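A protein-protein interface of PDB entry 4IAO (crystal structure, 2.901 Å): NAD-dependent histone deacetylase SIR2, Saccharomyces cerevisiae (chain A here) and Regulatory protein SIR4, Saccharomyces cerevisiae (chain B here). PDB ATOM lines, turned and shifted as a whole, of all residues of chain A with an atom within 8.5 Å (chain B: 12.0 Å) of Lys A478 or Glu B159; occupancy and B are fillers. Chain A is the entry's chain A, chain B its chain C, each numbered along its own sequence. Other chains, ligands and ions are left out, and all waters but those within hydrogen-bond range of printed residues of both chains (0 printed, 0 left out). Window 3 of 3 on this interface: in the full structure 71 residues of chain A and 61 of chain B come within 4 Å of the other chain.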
ATOM      1  N   ARG A 167      19.120 -26.543  12.917  1.00  0.00           N
ATOM      2  CA  ARG A 167      19.096 -25.480  13.928  1.00  0.00           C
ATOM      3  C   ARG A 167      19.687 -24.178  13.398  1.00  0.00           C
ATOM      4  O   ARG A 167      20.672 -24.190  12.658  1.00  0.00           O
ATOM      5  CB  ARG A 167      19.851 -25.903  15.190  1.00  0.00           C
ATOM      6  CG  ARG A 167      19.658 -27.350  15.593  1.00  0.00           C
ATOM      7  CD  ARG A 167      19.315 -27.469  17.073  1.00  0.00           C
ATOM      8  NE  ARG A 167      20.461 -27.803  17.920  1.00  0.00           N
ATOM      9  CZ  ARG A 167      21.031 -26.964  18.780  1.00  0.00           C
ATOM     10  NH1 ARG A 167      20.578 -25.719  18.904  1.00  0.00           N
ATOM     11  NH2 ARG A 167      22.059 -27.366  19.517  1.00  0.00           N
ATOM     12  N   SER A 169      21.893 -21.076  13.264  1.00  0.00           N
ATOM     13  CA  SER A 169      23.226 -20.801  13.790  1.00  0.00           C
ATOM     14  C   SER A 169      23.263 -19.507  14.599  1.00  0.00           C
ATOM     15  O   SER A 169      24.120 -19.340  15.469  1.00  0.00           O
ATOM     16  CB  SER A 169      24.243 -20.706  12.657  1.00  0.00           C
ATOM     17  OG  SER A 169      24.075 -19.492  11.945  1.00  0.00           O
ATOM     18  N   PHE A 171      20.586 -18.330  16.444  1.00  0.00           N
ATOM     19  CA  PHE A 171      19.806 -18.414  17.677  1.00  0.00           C
ATOM     20  C   PHE A 171      20.276 -19.633  18.473  1.00  0.00           C
ATOM     21  O   PHE A 171      19.769 -20.736  18.281  1.00  0.00           O
ATOM     22  CB  PHE A 171      18.355 -18.638  17.248  1.00  0.00           C
ATOM     23  CG  PHE A 171      17.334 -18.284  18.278  1.00  0.00           C
ATOM     24  CD1 PHE A 171      16.436 -17.256  18.037  1.00  0.00           C
ATOM     25  CD2 PHE A 171      17.235 -19.003  19.457  1.00  0.00           C
ATOM     26  CE1 PHE A 171      15.471 -16.927  18.969  1.00  0.00           C
ATOM     27  CE2 PHE A 171      16.278 -18.681  20.395  1.00  0.00           C
ATOM     28  CZ  PHE A 171      15.391 -17.643  20.149  1.00  0.00           C
ATOM     29  N   PHE A 172      21.258 -19.441  19.349  1.00  0.00           N
ATOM     30  CA  PHE A 172      21.668 -20.456  20.319  1.00  0.00           C
ATOM     31  C   PHE A 172      21.579 -20.157  21.816  1.00  0.00           C
ATOM     32  O   PHE A 172      22.014 -20.974  22.624  1.00  0.00           O
ATOM     33  CB  PHE A 172      23.015 -21.064  19.955  1.00  0.00           C
ATOM     34  CG  PHE A 172      24.117 -20.075  19.881  1.00  0.00           C
ATOM     35  CD1 PHE A 172      24.990 -19.918  20.940  1.00  0.00           C
ATOM     36  CD2 PHE A 172      24.285 -19.298  18.749  1.00  0.00           C
ATOM     37  CE1 PHE A 172      26.011 -19.008  20.871  1.00  0.00           C
ATOM     38  CE2 PHE A 172      25.302 -18.381  18.675  1.00  0.00           C
ATOM     39  CZ  PHE A 172      26.168 -18.233  19.735  1.00  0.00           C
ATOM     40  N   THR A 173      21.108 -18.978  22.202  1.00  0.00           N
ATOM     41  CA  THR A 173      21.357 -18.537  23.578  1.00  0.00           C
ATOM     42  C   THR A 173      20.205 -17.826  24.269  1.00  0.00           C
ATOM     43  O   THR A 173      19.283 -17.319  23.624  1.00  0.00           O
ATOM     44  CB  THR A 173      22.603 -17.623  23.661  1.00  0.00           C
ATOM     45  OG1 THR A 173      23.226 -17.781  24.939  1.00  0.00           O
ATOM     46  CG2 THR A 173      22.218 -16.167  23.481  1.00  0.00           C
ATOM     47  N   PHE A 435      15.703 -28.446  18.681  1.00  0.00           N
ATOM     48  CA  PHE A 435      15.288 -27.180  19.263  1.00  0.00           C
ATOM     49  C   PHE A 435      16.462 -26.214  19.274  1.00  0.00           C
ATOM     50  O   PHE A 435      17.549 -26.565  19.731  1.00  0.00           O
ATOM     51  CB  PHE A 435      14.772 -27.385  20.688  1.00  0.00           C
ATOM     52  CG  PHE A 435      13.318 -27.762  20.769  1.00  0.00           C
ATOM     53  CD1 PHE A 435      12.938 -29.078  20.982  1.00  0.00           C
ATOM     54  CD2 PHE A 435      12.331 -26.800  20.655  1.00  0.00           C
ATOM     55  CE1 PHE A 435      11.597 -29.428  21.067  1.00  0.00           C
ATOM     56  CE2 PHE A 435      10.997 -27.144  20.732  1.00  0.00           C
ATOM     57  CZ  PHE A 435      10.631 -28.461  20.941  1.00  0.00           C
ATOM     58  N   ASP A 436      16.242 -25.003  18.769  1.00  0.00           N
ATOM     59  CA  ASP A 436      17.291 -23.994  18.731  1.00  0.00           C
ATOM     60  C   ASP A 436      17.803 -23.737  20.128  1.00  0.00           C
ATOM     61  O   ASP A 436      19.002 -23.602  20.353  1.00  0.00           O
ATOM     62  CB  ASP A 436      16.762 -22.690  18.147  1.00  0.00           C
ATOM     63  CG  ASP A 436      16.397 -22.820  16.697  1.00  0.00           C
ATOM     64  OD1 ASP A 436      17.148 -23.498  15.963  1.00  0.00           O
ATOM     65  OD2 ASP A 436      15.360 -22.256  16.293  1.00  0.00           O
ATOM     66  N   LEU A 437      16.874 -23.669  21.071  1.00  0.00           N
ATOM     67  CA  LEU A 437      17.232 -23.397  22.448  1.00  0.00           C
ATOM     68  C   LEU A 437      16.373 -24.210  23.403  1.00  0.00           C
ATOM     69  O   LEU A 437      15.146 -24.197  23.317  1.00  0.00           O
ATOM     70  CB  LEU A 437      17.069 -21.909  22.743  1.00  0.00           C
ATOM     71  CG  LEU A 437      17.356 -21.564  24.199  1.00  0.00           C
ATOM     72  CD1 LEU A 437      18.853 -21.608  24.447  1.00  0.00           C
ATOM     73  CD2 LEU A 437      16.759 -20.216  24.562  1.00  0.00           C
ATOM     74  N   SER A 438      17.020 -24.896  24.335  1.00  0.00           N
ATOM     75  CA  SER A 438      16.294 -25.727  25.275  1.00  0.00           C
ATOM     76  C   SER A 438      16.684 -25.374  26.694  1.00  0.00           C
ATOM     77  O   SER A 438      17.808 -25.626  27.115  1.00  0.00           O
ATOM     78  CB  SER A 438      16.598 -27.198  25.009  1.00  0.00           C
ATOM     79  OG  SER A 438      16.921 -27.393  23.642  1.00  0.00           O
ATOM     80  N   GLU A 475      25.068 -23.485  31.186  1.00  0.00           N
ATOM     81  CA  GLU A 475      25.042 -24.016  29.825  1.00  0.00           C
ATOM     82  C   GLU A 475      25.731 -25.384  29.768  1.00  0.00           C
ATOM     83  O   GLU A 475      26.928 -25.491  30.024  1.00  0.00           O
ATOM     84  CB  GLU A 475      25.729 -23.019  28.877  1.00  0.00           C
ATOM     85  CG  GLU A 475      26.168 -23.570  27.528  1.00  0.00           C
ATOM     86  CD  GLU A 475      26.958 -22.553  26.717  1.00  0.00           C
ATOM     87  OE1 GLU A 475      26.724 -21.337  26.897  1.00  0.00           O
ATOM     88  OE2 GLU A 475      27.820 -22.969  25.909  1.00  0.00           O
ATOM     89  N   LYS A 476      24.973 -26.430  29.443  1.00  0.00           N
ATOM     90  CA  LYS A 476      25.555 -27.767  29.325  1.00  0.00           C
ATOM     91  C   LYS A 476      25.985 -28.124  27.902  1.00  0.00           C
ATOM     92  O   LYS A 476      26.755 -29.061  27.702  1.00  0.00           O
ATOM     93  CB  LYS A 476      24.596 -28.828  29.872  1.00  0.00           C
ATOM     94  CG  LYS A 476      24.305 -28.700  31.361  1.00  0.00           C
ATOM     95  CD  LYS A 476      25.577 -28.744  32.196  1.00  0.00           C
ATOM     96  CE  LYS A 476      25.268 -28.641  33.683  1.00  0.00           C
ATOM     97  NZ  LYS A 476      26.495 -28.407  34.498  1.00  0.00           N
ATOM     98  N   ASP A 477      25.503 -27.354  26.931  1.00  0.00           N
ATOM     99  CA  ASP A 477      25.858 -27.521  25.522  1.00  0.00           C
ATOM    100  C   ASP A 477      25.340 -26.306  24.775  1.00  0.00           C
ATOM    101  O   ASP A 477      24.680 -25.454  25.363  1.00  0.00           O
ATOM    102  CB  ASP A 477      25.244 -28.792  24.930  1.00  0.00           C
ATOM    103  CG  ASP A 477      26.175 -29.993  25.013  1.00  0.00           C
ATOM    104  OD1 ASP A 477      25.677 -31.115  25.243  1.00  0.00           O
ATOM    105  OD2 ASP A 477      27.400 -29.818  24.848  1.00  0.00           O
ATOM    106  N   LYS A 478      25.617 -26.224  23.481  1.00  0.00           N
ATOM    107  CA  LYS A 478      25.175 -25.065  22.717  1.00  0.00           C
ATOM    108  C   LYS A 478      23.662 -25.133  22.573  1.00  0.00           C
ATOM    109  O   LYS A 478      23.120 -26.143  22.116  1.00  0.00           O
ATOM    110  CB  LYS A 478      25.861 -25.014  21.348  1.00  0.00           C
ATOM    111  CG  LYS A 478      26.736 -23.784  21.131  1.00  0.00           C
ATOM    112  CD  LYS A 478      27.776 -23.623  22.237  1.00  0.00           C
ATOM    113  CE  LYS A 478      28.487 -22.273  22.149  1.00  0.00           C
ATOM    114  NZ  LYS A 478      29.379 -22.023  23.321  1.00  0.00           N
ATOM    115  N   GLY A 479      22.983 -24.070  22.992  1.00  0.00           N
ATOM    116  CA  GLY A 479      21.530 -24.033  22.965  1.00  0.00           C
ATOM    117  C   GLY A 479      20.859 -24.828  24.074  1.00  0.00           C
ATOM    118  O   GLY A 479      19.646 -25.033  24.060  1.00  0.00           O
ATOM    119  N   VAL A 480      21.655 -25.275  25.038  1.00  0.00           N
ATOM    120  CA  VAL A 480      21.147 -26.057  26.159  1.00  0.00           C
ATOM    121  C   VAL A 480      21.561 -25.432  27.498  1.00  0.00           C
ATOM    122  O   VAL A 480      22.744 -25.222  27.757  1.00  0.00           O
ATOM    123  CB  VAL A 480      21.647 -27.516  26.094  1.00  0.00           C
ATOM    124  CG1 VAL A 480      21.147 -28.306  27.284  1.00  0.00           C
ATOM    125  CG2 VAL A 480      21.212 -28.166  24.792  1.00  0.00           C
ATOM    126  N   TYR A 481      20.574 -25.138  28.341  1.00  0.00           N
ATOM    127  CA  TYR A 481      20.811 -24.497  29.628  1.00  0.00           C
ATOM    128  C   TYR A 481      20.015 -25.157  30.752  1.00  0.00           C
ATOM    129  O   TYR A 481      18.833 -25.451  30.593  1.00  0.00           O
ATOM    130  CB  TYR A 481      20.410 -23.024  29.561  1.00  0.00           C
ATOM    131  CG  TYR A 481      21.276 -22.165  28.678  1.00  0.00           C
ATOM    132  CD1 TYR A 481      20.974 -21.994  27.337  1.00  0.00           C
ATOM    133  CD2 TYR A 481      22.386 -21.511  29.192  1.00  0.00           C
ATOM    134  CE1 TYR A 481      21.759 -21.197  26.526  1.00  0.00           C
ATOM    135  CE2 TYR A 481      23.177 -20.712  28.391  1.00  0.00           C
ATOM    136  CZ  TYR A 481      22.861 -20.557  27.059  1.00  0.00           C
ATOM    137  OH  TYR A 481      23.653 -19.764  26.259  1.00  0.00           O
ATOM    138  N   PRO B 151      25.338 -36.024  13.995  1.00  0.00           N
ATOM    139  CA  PRO B 151      24.777 -34.701  14.279  1.00  0.00           C
ATOM    140  C   PRO B 151      25.806 -33.620  13.978  1.00  0.00           C
ATOM    141  O   PRO B 151      26.952 -33.714  14.429  1.00  0.00           O
ATOM    142  CB  PRO B 151      24.488 -34.755  15.782  1.00  0.00           C
ATOM    143  CG  PRO B 151      25.412 -35.806  16.312  1.00  0.00           C
ATOM    144  CD  PRO B 151      25.512 -36.829  15.218  1.00  0.00           C
ATOM    145  N   LEU B 152      25.394 -32.611  13.218  1.00  0.00           N
ATOM    146  CA  LEU B 152      26.274 -31.507  12.864  1.00  0.00           C
ATOM    147  C   LEU B 152      25.601 -30.171  13.155  1.00  0.00           C
ATOM    148  O   LEU B 152      24.582 -29.831  12.549  1.00  0.00           O
ATOM    149  CB  LEU B 152      26.656 -31.575  11.385  1.00  0.00           C
ATOM    150  CG  LEU B 152      27.368 -32.830  10.885  1.00  0.00           C
ATOM    151  CD1 LEU B 152      27.822 -32.624   9.443  1.00  0.00           C
ATOM    152  CD2 LEU B 152      28.542 -33.179  11.784  1.00  0.00           C
ATOM    153  N   TYR B 153      26.176 -29.415  14.082  1.00  0.00           N
ATOM    154  CA  TYR B 153      25.666 -28.088  14.393  1.00  0.00           C
ATOM    155  C   TYR B 153      26.813 -27.110  14.598  1.00  0.00           C
ATOM    156  O   TYR B 153      27.731 -27.360  15.387  1.00  0.00           O
ATOM    157  CB  TYR B 153      24.776 -28.137  15.634  1.00  0.00           C
ATOM    158  CG  TYR B 153      24.143 -26.818  16.006  1.00  0.00           C
ATOM    159  CD1 TYR B 153      23.506 -26.039  15.052  1.00  0.00           C
ATOM    160  CD2 TYR B 153      24.168 -26.360  17.316  1.00  0.00           C
ATOM    161  CE1 TYR B 153      22.927 -24.830  15.389  1.00  0.00           C
ATOM    162  CE2 TYR B 153      23.582 -25.153  17.665  1.00  0.00           C
ATOM    163  CZ  TYR B 153      22.958 -24.395  16.697  1.00  0.00           C
ATOM    164  OH  TYR B 153      22.368 -23.196  17.034  1.00  0.00           O
ATOM    165  N   ALA B 154      26.752 -25.999  13.873  1.00  0.00           N
ATOM    166  CA  ALA B 154      27.730 -24.934  14.028  1.00  0.00           C
ATOM    167  C   ALA B 154      27.035 -23.648  14.465  1.00  0.00           C
ATOM    168  O   ALA B 154      25.943 -23.329  13.998  1.00  0.00           O
ATOM    169  CB  ALA B 154      28.490 -24.723  12.734  1.00  0.00           C
ATOM    170  N   VAL B 155      27.675 -22.911  15.361  1.00  0.00           N
ATOM    171  CA  VAL B 155      27.117 -21.662  15.848  1.00  0.00           C
ATOM    172  C   VAL B 155      27.990 -20.504  15.408  1.00  0.00           C
ATOM    173  O   VAL B 155      29.172 -20.690  15.127  1.00  0.00           O
ATOM    174  CB  VAL B 155      27.043 -21.650  17.381  1.00  0.00           C
ATOM    175  CG1 VAL B 155      25.816 -22.397  17.859  1.00  0.00           C
ATOM    176  CG2 VAL B 155      28.309 -22.249  17.973  1.00  0.00           C
ATOM    177  N   SER B 156      27.401 -19.313  15.333  1.00  0.00           N
ATOM    178  CA  SER B 156      28.175 -18.104  15.101  1.00  0.00           C
ATOM    179  C   SER B 156      28.312 -17.451  16.449  1.00  0.00           C
ATOM    180  O   SER B 156      27.360 -16.868  16.958  1.00  0.00           O
ATOM    181  CB  SER B 156      27.434 -17.160  14.155  1.00  0.00           C
ATOM    182  OG  SER B 156      27.068 -17.818  12.951  1.00  0.00           O
ATOM    183  N   THR B 157      29.502 -17.523  17.026  1.00  0.00           N
ATOM    184  CA  THR B 157      29.671 -17.042  18.387  1.00  0.00           C
ATOM    185  C   THR B 157      30.879 -16.137  18.562  1.00  0.00           C
ATOM    186  O   THR B 157      31.867 -16.237  17.835  1.00  0.00           O
ATOM    187  CB  THR B 157      29.742 -18.202  19.403  1.00  0.00           C
ATOM    188  OG1 THR B 157      29.602 -17.681  20.731  1.00  0.00           O
ATOM    189  CG2 THR B 157      31.059 -18.959  19.279  1.00  0.00           C
ATOM    190  N   PHE B 158      30.778 -15.247  19.543  1.00  0.00           N
ATOM    191  CA  PHE B 158      31.831 -14.288  19.847  1.00  0.00           C
ATOM    192  C   PHE B 158      32.754 -14.800  20.954  1.00  0.00           C
ATOM    193  O   PHE B 158      33.651 -14.084  21.398  1.00  0.00           O
ATOM    194  CB  PHE B 158      31.218 -12.935  20.225  1.00  0.00           C
ATOM    195  CG  PHE B 158      30.529 -12.240  19.081  1.00  0.00           C
ATOM    196  CD1 PHE B 158      31.108 -11.140  18.474  1.00  0.00           C
ATOM    197  CD2 PHE B 158      29.312 -12.697  18.603  1.00  0.00           C
ATOM    198  CE1 PHE B 158      30.484 -10.504  17.425  1.00  0.00           C
ATOM    199  CE2 PHE B 158      28.684 -12.065  17.547  1.00  0.00           C
ATOM    200  CZ  PHE B 158      29.270 -10.965  16.960  1.00  0.00           C
ATOM    201  N   GLU B 159      32.520 -16.037  21.397  1.00  0.00           N
ATOM    202  CA  GLU B 159      33.329 -16.673  22.439  1.00  0.00           C
ATOM    203  C   GLU B 159      34.823 -16.546  22.156  1.00  0.00           C
ATOM    204  O   GLU B 159      35.259 -16.639  21.006  1.00  0.00           O
ATOM    205  CB  GLU B 159      32.977 -18.159  22.572  1.00  0.00           C
ATOM    206  CG  GLU B 159      31.543 -18.458  22.996  1.00  0.00           C
ATOM    207  CD  GLU B 159      31.321 -18.353  24.496  1.00  0.00           C
ATOM    208  OE1 GLU B 159      32.235 -17.886  25.211  1.00  0.00           O
ATOM    209  OE2 GLU B 159      30.226 -18.748  24.959  1.00  0.00           O
ATOM    210  OXT GLU B 159      35.622 -16.348  23.071  1.00  0.00           O
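Of the printed residues of chain B, Phe A171 touches Tyr B153 (3.8 Å).
Ser A438 touches none of the printed residues of chain B.
Glu A475 touches none of the printed residues of chain B.
No residue of chain B comes within 4 Å of Asp A477.
Lys A478 touches two residues of chain B.
Val A480 touches none of the printed residues of chain B.
Pro B151 touches none of the printed residues of chain A.
Of the printed residues of chain A, Ala B154 touches Ser A169.
Of chain A, only Lys A478 comes within 4 Å of Glu B159.
The nearest residue of chain B that does not touch Lys A478 is Tyr B153 (4.3 Å).
The nearest residue of chain A that does not touch Glu B159 is Glu A475 (4.8 Å).
NH2 of Arg A167 touches CD2 of Tyr B153, 3.2 Å away.
Ser A169 touches Ala B154 (CB to O, 3.4 Å).
Val B155 touches Ser A169.
OH of Tyr B153 touches O of Phe A171, at 3.8 Å.
OH of Tyr B153 touches CB of Phe A172 (3.7 Å).
CG1 of Val B155 touches CG of Phe A172, at 3.5 Å.
Ser B156 touches Phe A172.
Phe A172 touches Thr B157 (CZ to CB, 3.6 Å).
Lys A478 touches Val B155 (CG to CG1, 3.7 Å).
The backbone carbonyl oxygen (O) of Lys A478 sits at hydrogen-bond distance from the guanidinium group (NH2) of Arg A167, 3.1 Å away.
The backbone carbonyl oxygen (O) of Phe A172 sits close to the backbone NH (N) of Gly A479.
NH1 of Arg A167 is in hydrogen-bond range of O of Asp A436 (3.0 Å).
The side-chain amino group (NZ) of Lys A478 is in salt-bridge range of the side-chain carboxylate (OE2) of Glu A475.
The backbone NH (N) of Glu B159 sits close to the side-chain hydroxyl (OG1) of Thr B157 (3.4 Å).
The guanidinium group (NH1) of Arg A167 lies within hydrogen-bond range of the backbone carbonyl oxygen (O) of Phe A435 (3.3 Å).
Of the 16 printed residues of chain A, 5 touch a printed residue of chain B.
Printed residues of chain A that touch a printed residue of chain B: Arg A167, Ser A169, Phe A171, Phe A172 and Lys A478.
Hydrophobic or aromatic side chains of chain A within 4 Å of the printed part of chain B: Phe A172.
Printed residues of chain B that touch a printed residue of chain A: Tyr B153, Ala B154, Val B155, Ser B156, Thr B157 and Glu B159.
Among the printed residues, 11 pairs touch across the chains.
NZ of Lys A478 is in salt-bridge range of OE2 of Glu B159, 3.8 Å away.
O of Ser A169 lies within hydrogen-bond range of N of Ser B156 (3.3 Å).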
